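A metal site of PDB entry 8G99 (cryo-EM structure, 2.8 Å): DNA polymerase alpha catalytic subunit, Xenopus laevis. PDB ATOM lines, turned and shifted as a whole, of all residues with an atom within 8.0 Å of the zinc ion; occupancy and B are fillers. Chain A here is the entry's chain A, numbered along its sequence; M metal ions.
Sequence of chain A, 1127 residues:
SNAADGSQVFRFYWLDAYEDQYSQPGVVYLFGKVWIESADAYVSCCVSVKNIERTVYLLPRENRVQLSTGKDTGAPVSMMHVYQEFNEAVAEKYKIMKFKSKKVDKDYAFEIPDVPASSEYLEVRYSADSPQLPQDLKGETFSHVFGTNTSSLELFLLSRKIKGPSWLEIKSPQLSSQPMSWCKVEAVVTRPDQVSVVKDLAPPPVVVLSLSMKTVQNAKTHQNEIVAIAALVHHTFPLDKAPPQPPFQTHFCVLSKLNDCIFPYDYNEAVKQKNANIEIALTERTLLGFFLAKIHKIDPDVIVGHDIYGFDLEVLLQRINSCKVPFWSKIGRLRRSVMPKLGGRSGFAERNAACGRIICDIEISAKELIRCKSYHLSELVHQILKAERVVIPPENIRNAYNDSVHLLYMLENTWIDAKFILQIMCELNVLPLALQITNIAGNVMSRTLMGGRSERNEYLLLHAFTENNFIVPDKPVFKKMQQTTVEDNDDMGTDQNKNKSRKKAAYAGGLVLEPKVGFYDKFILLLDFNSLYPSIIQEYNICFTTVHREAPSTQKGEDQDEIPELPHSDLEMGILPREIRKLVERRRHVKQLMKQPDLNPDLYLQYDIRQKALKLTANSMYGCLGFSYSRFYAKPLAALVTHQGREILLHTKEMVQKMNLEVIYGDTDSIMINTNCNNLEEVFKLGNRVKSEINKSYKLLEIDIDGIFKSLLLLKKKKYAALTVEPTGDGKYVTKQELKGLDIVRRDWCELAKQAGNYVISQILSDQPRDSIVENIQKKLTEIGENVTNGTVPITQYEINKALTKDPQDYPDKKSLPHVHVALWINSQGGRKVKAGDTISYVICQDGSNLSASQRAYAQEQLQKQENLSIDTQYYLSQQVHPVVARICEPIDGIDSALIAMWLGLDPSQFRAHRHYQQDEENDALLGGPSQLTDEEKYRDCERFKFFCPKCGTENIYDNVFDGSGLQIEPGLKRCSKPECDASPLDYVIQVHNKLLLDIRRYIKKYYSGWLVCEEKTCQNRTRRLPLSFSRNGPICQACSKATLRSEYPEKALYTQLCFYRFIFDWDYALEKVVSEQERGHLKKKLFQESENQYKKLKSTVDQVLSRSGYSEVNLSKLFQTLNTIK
The backbone NH (N) of Glu 1016 lies close to the side-chain sulfur (SG) of Cys 1014, 3.7 Å away.
The backbone carbonyl oxygen (O) of Asn 1021 sits at hydrogen-bond distance from the backbone NH (N) of Cys 1014 (2.9 Å).
N of Cys 1037 lies within hydrogen-bond range of O of Ala 1043, at 2.8 Å.
The side-chain sulfur (SG) of Cys 1019 sits close to the backbone NH (N) of Asn 1021 (3.6 Å).
The side-chain sulfur (SG) of Cys 1037 lies close to the backbone NH (N) of Ala 1039, 3.3 Å away.
Of the 22 residues printed, 4 come within 4 Å of the zinc ion.
SG of Cys 1040 is bound to the zinc ion, 2.3 Å away.
The side-chain sulfur (SG) of Cys 1037 is bound to the zinc ion (2.3 Å).
SG of Cys 1019 binds the zinc ion (2.3 Å).
The zinc ion is bound by SG of Cys 1014, at 2.3 Å.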
ATOM      1  N   VAL A 745       8.357  -3.192   4.141  1.00  0.00           N
ATOM      2  CA  VAL A 745       7.053  -3.741   3.743  1.00  0.00           C
ATOM      3  C   VAL A 745       6.371  -4.396   4.937  1.00  0.00           C
ATOM      4  O   VAL A 745       5.168  -4.225   5.153  1.00  0.00           O
ATOM      5  CB  VAL A 745       7.222  -4.722   2.576  1.00  0.00           C
ATOM      6  CG1 VAL A 745       5.868  -5.226   2.103  1.00  0.00           C
ATOM      7  CG2 VAL A 745       7.978  -4.062   1.427  1.00  0.00           C
ATOM      8  N   ARG A 746       7.128  -5.161   5.725  1.00  0.00           N
ATOM      9  CA  ARG A 746       6.573  -5.771   6.922  1.00  0.00           C
ATOM     10  C   ARG A 746       6.262  -4.697   7.951  1.00  0.00           C
ATOM     11  O   ARG A 746       7.083  -3.808   8.201  1.00  0.00           O
ATOM     12  CB  ARG A 746       7.559  -6.785   7.501  1.00  0.00           C
ATOM     13  CG  ARG A 746       7.368  -8.203   6.990  1.00  0.00           C
ATOM     14  CD  ARG A 746       7.624  -9.221   8.084  1.00  0.00           C
ATOM     15  NE  ARG A 746       9.010  -9.211   8.525  1.00  0.00           N
ATOM     16  CZ  ARG A 746       9.419  -9.536   9.744  1.00  0.00           C
ATOM     17  NH1 ARG A 746       8.563  -9.912  10.686  1.00  0.00           N
ATOM     18  NH2 ARG A 746      10.719  -9.485  10.029  1.00  0.00           N
ATOM     19  N   VAL A1013      16.293 -17.377  -0.098  1.00  0.00           N
ATOM     20  CA  VAL A1013      16.102 -16.432   0.997  1.00  0.00           C
ATOM     21  C   VAL A1013      16.163 -15.023   0.436  1.00  0.00           C
ATOM     22  O   VAL A1013      16.979 -14.728  -0.448  1.00  0.00           O
ATOM     23  CB  VAL A1013      17.151 -16.612   2.106  1.00  0.00           C
ATOM     24  CG1 VAL A1013      16.662 -15.999   3.395  1.00  0.00           C
ATOM     25  CG2 VAL A1013      17.477 -18.081   2.305  1.00  0.00           C
ATOM     26  N   CYS A1014      15.286 -14.151   0.919  1.00  0.00           N
ATOM     27  CA  CYS A1014      15.309 -12.757   0.510  1.00  0.00           C
ATOM     28  C   CYS A1014      16.559 -12.073   1.048  1.00  0.00           C
ATOM     29  O   CYS A1014      16.946 -12.262   2.205  1.00  0.00           O
ATOM     30  CB  CYS A1014      14.057 -12.039   1.009  1.00  0.00           C
ATOM     31  SG  CYS A1014      13.763 -10.451   0.237  1.00  0.00           S
ATOM     32  N   GLU A1015      17.205 -11.279   0.198  1.00  0.00           N
ATOM     33  CA  GLU A1015      18.418 -10.577   0.603  1.00  0.00           C
ATOM     34  C   GLU A1015      18.122  -9.427   1.557  1.00  0.00           C
ATOM     35  O   GLU A1015      19.036  -8.931   2.215  1.00  0.00           O
ATOM     36  CB  GLU A1015      19.156 -10.061  -0.622  1.00  0.00           C
ATOM     37  CG  GLU A1015      18.551  -8.821  -1.247  1.00  0.00           C
ATOM     38  CD  GLU A1015      19.068  -8.562  -2.646  1.00  0.00           C
ATOM     39  OE1 GLU A1015      20.094  -9.173  -3.024  1.00  0.00           O
ATOM     40  OE2 GLU A1015      18.451  -7.752  -3.369  1.00  0.00           O
ATOM     41  N   GLU A1016      16.873  -8.984   1.637  1.00  0.00           N
ATOM     42  CA  GLU A1016      16.519  -7.901   2.543  1.00  0.00           C
ATOM     43  C   GLU A1016      16.493  -8.395   3.984  1.00  0.00           C
ATOM     44  O   GLU A1016      15.851  -9.404   4.293  1.00  0.00           O
ATOM     45  CB  GLU A1016      15.161  -7.317   2.166  1.00  0.00           C
ATOM     46  CG  GLU A1016      14.698  -6.161   3.039  1.00  0.00           C
ATOM     47  CD  GLU A1016      15.723  -5.055   3.146  1.00  0.00           C
ATOM     48  OE1 GLU A1016      16.674  -5.204   3.929  1.00  0.00           O
ATOM     49  OE2 GLU A1016      15.575  -4.038   2.437  1.00  0.00           O
ATOM     50  N   LYS A1017      17.212  -7.689   4.869  1.00  0.00           N
ATOM     51  CA  LYS A1017      17.274  -8.104   6.265  1.00  0.00           C
ATOM     52  C   LYS A1017      15.902  -8.042   6.918  1.00  0.00           C
ATOM     53  O   LYS A1017      15.568  -8.885   7.755  1.00  0.00           O
ATOM     54  CB  LYS A1017      18.263  -7.218   7.021  1.00  0.00           C
ATOM     55  CG  LYS A1017      19.711  -7.472   6.663  1.00  0.00           C
ATOM     56  CD  LYS A1017      20.513  -7.892   7.883  1.00  0.00           C
ATOM     57  CE  LYS A1017      21.916  -8.348   7.504  1.00  0.00           C
ATOM     58  NZ  LYS A1017      22.532  -7.486   6.458  1.00  0.00           N
ATOM     59  N   THR A1018      15.096  -7.047   6.554  1.00  0.00           N
ATOM     60  CA  THR A1018      13.798  -6.826   7.164  1.00  0.00           C
ATOM     61  C   THR A1018      12.716  -7.736   6.599  1.00  0.00           C
ATOM     62  O   THR A1018      11.579  -7.699   7.092  1.00  0.00           O
ATOM     63  CB  THR A1018      13.382  -5.368   6.995  1.00  0.00           C
ATOM     64  OG1 THR A1018      13.748  -4.912   5.688  1.00  0.00           O
ATOM     65  CG2 THR A1018      14.064  -4.511   8.037  1.00  0.00           C
ATOM     66  N   CYS A1019      13.016  -8.542   5.580  1.00  0.00           N
ATOM     67  CA  CYS A1019      12.078  -9.508   5.040  1.00  0.00           C
ATOM     68  C   CYS A1019      12.524 -10.942   5.294  1.00  0.00           C
ATOM     69  O   CYS A1019      11.810 -11.711   5.937  1.00  0.00           O
ATOM     70  CB  CYS A1019      11.895  -9.270   3.532  1.00  0.00           C
ATOM     71  SG  CYS A1019      10.958 -10.533   2.670  1.00  0.00           S
ATOM     72  N   GLN A1020      13.720 -11.310   4.826  1.00  0.00           N
ATOM     73  CA  GLN A1020      14.277 -12.653   5.059  1.00  0.00           C
ATOM     74  C   GLN A1020      13.245 -13.743   4.801  1.00  0.00           C
ATOM     75  O   GLN A1020      13.132 -14.717   5.542  1.00  0.00           O
ATOM     76  CB  GLN A1020      14.849 -12.755   6.472  1.00  0.00           C
ATOM     77  CG  GLN A1020      16.291 -12.295   6.590  1.00  0.00           C
ATOM     78  CD  GLN A1020      16.793 -12.313   8.013  1.00  0.00           C
ATOM     79  OE1 GLN A1020      17.469 -13.251   8.428  1.00  0.00           O
ATOM     80  NE2 GLN A1020      16.478 -11.263   8.772  1.00  0.00           N
ATOM     81  N   ASN A1021      12.487 -13.595   3.718  1.00  0.00           N
ATOM     82  CA  ASN A1021      11.510 -14.591   3.347  1.00  0.00           C
ATOM     83  C   ASN A1021      12.211 -15.823   2.779  1.00  0.00           C
ATOM     84  O   ASN A1021      13.070 -15.710   1.907  1.00  0.00           O
ATOM     85  CB  ASN A1021      10.525 -14.026   2.323  1.00  0.00           C
ATOM     86  CG  ASN A1021       9.438 -15.004   1.948  1.00  0.00           C
ATOM     87  OD1 ASN A1021       9.230 -15.303   0.774  1.00  0.00           O
ATOM     88  ND2 ASN A1021       8.719 -15.501   2.951  1.00  0.00           N
ATOM     89  N   ARG A1022      11.833 -16.991   3.283  1.00  0.00           N
ATOM     90  CA  ARG A1022      12.453 -18.257   2.892  1.00  0.00           C
ATOM     91  C   ARG A1022      11.413 -19.111   2.177  1.00  0.00           C
ATOM     92  O   ARG A1022      10.403 -19.489   2.771  1.00  0.00           O
ATOM     93  CB  ARG A1022      12.996 -18.987   4.116  1.00  0.00           C
ATOM     94  CG  ARG A1022      14.214 -19.841   3.839  1.00  0.00           C
ATOM     95  CD  ARG A1022      14.721 -20.502   5.098  1.00  0.00           C
ATOM     96  NE  ARG A1022      15.526 -21.685   4.803  1.00  0.00           N
ATOM     97  CZ  ARG A1022      15.123 -22.937   4.960  1.00  0.00           C
ATOM     98  NH1 ARG A1022      13.912 -23.227   5.391  1.00  0.00           N
ATOM     99  NH2 ARG A1022      15.964 -23.931   4.668  1.00  0.00           N
ATOM    100  N   ILE A1036      12.286 -11.959  -8.022  1.00  0.00           N
ATOM    101  CA  ILE A1036      11.755 -10.937  -7.129  1.00  0.00           C
ATOM    102  C   ILE A1036      11.018 -11.619  -5.995  1.00  0.00           C
ATOM    103  O   ILE A1036      10.129 -12.453  -6.232  1.00  0.00           O
ATOM    104  CB  ILE A1036      10.829  -9.969  -7.895  1.00  0.00           C
ATOM    105  CG1 ILE A1036      11.618  -9.182  -8.934  1.00  0.00           C
ATOM    106  CG2 ILE A1036      10.139  -9.029  -6.931  1.00  0.00           C
ATOM    107  CD1 ILE A1036      10.766  -8.603 -10.039  1.00  0.00           C
ATOM    108  N   CYS A1037      11.380 -11.285  -4.758  1.00  0.00           N
ATOM    109  CA  CYS A1037      10.729 -11.879  -3.604  1.00  0.00           C
ATOM    110  C   CYS A1037       9.259 -11.495  -3.581  1.00  0.00           C
ATOM    111  O   CYS A1037       8.905 -10.318  -3.658  1.00  0.00           O
ATOM    112  CB  CYS A1037      11.416 -11.421  -2.319  1.00  0.00           C
ATOM    113  SG  CYS A1037      10.478 -11.720  -0.816  1.00  0.00           S
ATOM    114  N   GLN A1038       8.391 -12.499  -3.472  1.00  0.00           N
ATOM    115  CA  GLN A1038       6.956 -12.272  -3.525  1.00  0.00           C
ATOM    116  C   GLN A1038       6.372 -11.883  -2.176  1.00  0.00           C
ATOM    117  O   GLN A1038       5.167 -11.607  -2.100  1.00  0.00           O
ATOM    118  CB  GLN A1038       6.250 -13.512  -4.054  1.00  0.00           C
ATOM    119  CG  GLN A1038       6.619 -13.864  -5.486  1.00  0.00           C
ATOM    120  CD  GLN A1038       6.424 -12.719  -6.445  1.00  0.00           C
ATOM    121  OE1 GLN A1038       5.306 -12.260  -6.656  1.00  0.00           O
ATOM    122  NE2 GLN A1038       7.513 -12.248  -7.041  1.00  0.00           N
ATOM    123  N   ALA A1039       7.180 -11.843  -1.128  1.00  0.00           N
ATOM    124  CA  ALA A1039       6.697 -11.360   0.166  1.00  0.00           C
ATOM    125  C   ALA A1039       6.740  -9.835   0.230  1.00  0.00           C
ATOM    126  O   ALA A1039       5.790  -9.202   0.693  1.00  0.00           O
ATOM    127  CB  ALA A1039       7.526 -11.973   1.300  1.00  0.00           C
ATOM    128  N   CYS A1040       7.848  -9.242  -0.223  1.00  0.00           N
ATOM    129  CA  CYS A1040       8.004  -7.791  -0.214  1.00  0.00           C
ATOM    130  C   CYS A1040       7.961  -7.171  -1.598  1.00  0.00           C
ATOM    131  O   CYS A1040       7.697  -5.960  -1.702  1.00  0.00           O
ATOM    132  CB  CYS A1040       9.324  -7.408   0.466  1.00  0.00           C
ATOM    133  SG  CYS A1040      10.801  -8.172  -0.233  1.00  0.00           S
ATOM    134  N   SER A1041       8.221  -7.934  -2.659  1.00  0.00           N
ATOM    135  CA  SER A1041       8.158  -7.457  -4.032  1.00  0.00           C
ATOM    136  C   SER A1041       9.201  -6.390  -4.336  1.00  0.00           C
ATOM    137  O   SER A1041       9.058  -5.652  -5.312  1.00  0.00           O
ATOM    138  CB  SER A1041       6.758  -6.931  -4.360  1.00  0.00           C
ATOM    139  OG  SER A1041       5.776  -7.914  -4.112  1.00  0.00           O
ATOM    140  N   LYS A1042      10.258  -6.301  -3.537  1.00  0.00           N
ATOM    141  CA  LYS A1042      11.241  -5.252  -3.692  1.00  0.00           C
ATOM    142  C   LYS A1042      12.683  -5.723  -3.514  1.00  0.00           C
ATOM    143  O   LYS A1042      13.589  -4.887  -3.553  1.00  0.00           O
ATOM    144  CB  LYS A1042      10.971  -4.111  -2.691  1.00  0.00           C
ATOM    145  CG  LYS A1042       9.597  -3.467  -2.856  1.00  0.00           C
ATOM    146  CD  LYS A1042       9.334  -2.462  -1.755  1.00  0.00           C
ATOM    147  CE  LYS A1042       7.995  -1.763  -1.953  1.00  0.00           C
ATOM    148  NZ  LYS A1042       7.692  -0.816  -0.847  1.00  0.00           N
ATOM    149  N   ALA A1043      12.922  -7.014  -3.333  1.00  0.00           N
ATOM    150  CA  ALA A1043      14.263  -7.531  -3.103  1.00  0.00           C
ATOM    151  C   ALA A1043      14.427  -8.848  -3.830  1.00  0.00           C
ATOM    152  O   ALA A1043      13.449  -9.494  -4.230  1.00  0.00           O
ATOM    153  CB  ALA A1043      14.543  -7.692  -1.605  1.00  0.00           C
ATOM    154  N   THR A1044      15.677  -9.247  -4.016  1.00  0.00           N
ATOM    155  CA  THR A1044      16.006 -10.432  -4.792  1.00  0.00           C
ATOM    156  C   THR A1044      16.143 -11.653  -3.901  1.00  0.00           C
ATOM    157  O   THR A1044      16.606 -11.579  -2.762  1.00  0.00           O
ATOM    158  CB  THR A1044      17.298 -10.214  -5.568  1.00  0.00           C
ATOM    159  OG1 THR A1044      17.198  -9.020  -6.347  1.00  0.00           O
ATOM    160  CG2 THR A1044      17.578 -11.386  -6.488  1.00  0.00           C
ATOM    161  N   LEU A1045      15.718 -12.798  -4.437  1.00  0.00           N
ATOM    162  CA  LEU A1045      15.870 -14.080  -3.759  1.00  0.00           C
ATOM    163  C   LEU A1045      17.210 -14.690  -4.140  1.00  0.00           C
ATOM    164  O   LEU A1045      17.529 -14.818  -5.321  1.00  0.00           O
ATOM    165  CB  LEU A1045      14.731 -15.028  -4.151  1.00  0.00           C
ATOM    166  CG  LEU A1045      13.338 -14.689  -3.618  1.00  0.00           C
ATOM    167  CD1 LEU A1045      12.303 -15.465  -4.398  1.00  0.00           C
ATOM    168  CD2 LEU A1045      13.245 -15.004  -2.148  1.00  0.00           C
HETATM  169 ZN    ZN M   1      11.511 -10.190   0.485  1.00  0.00          ZN
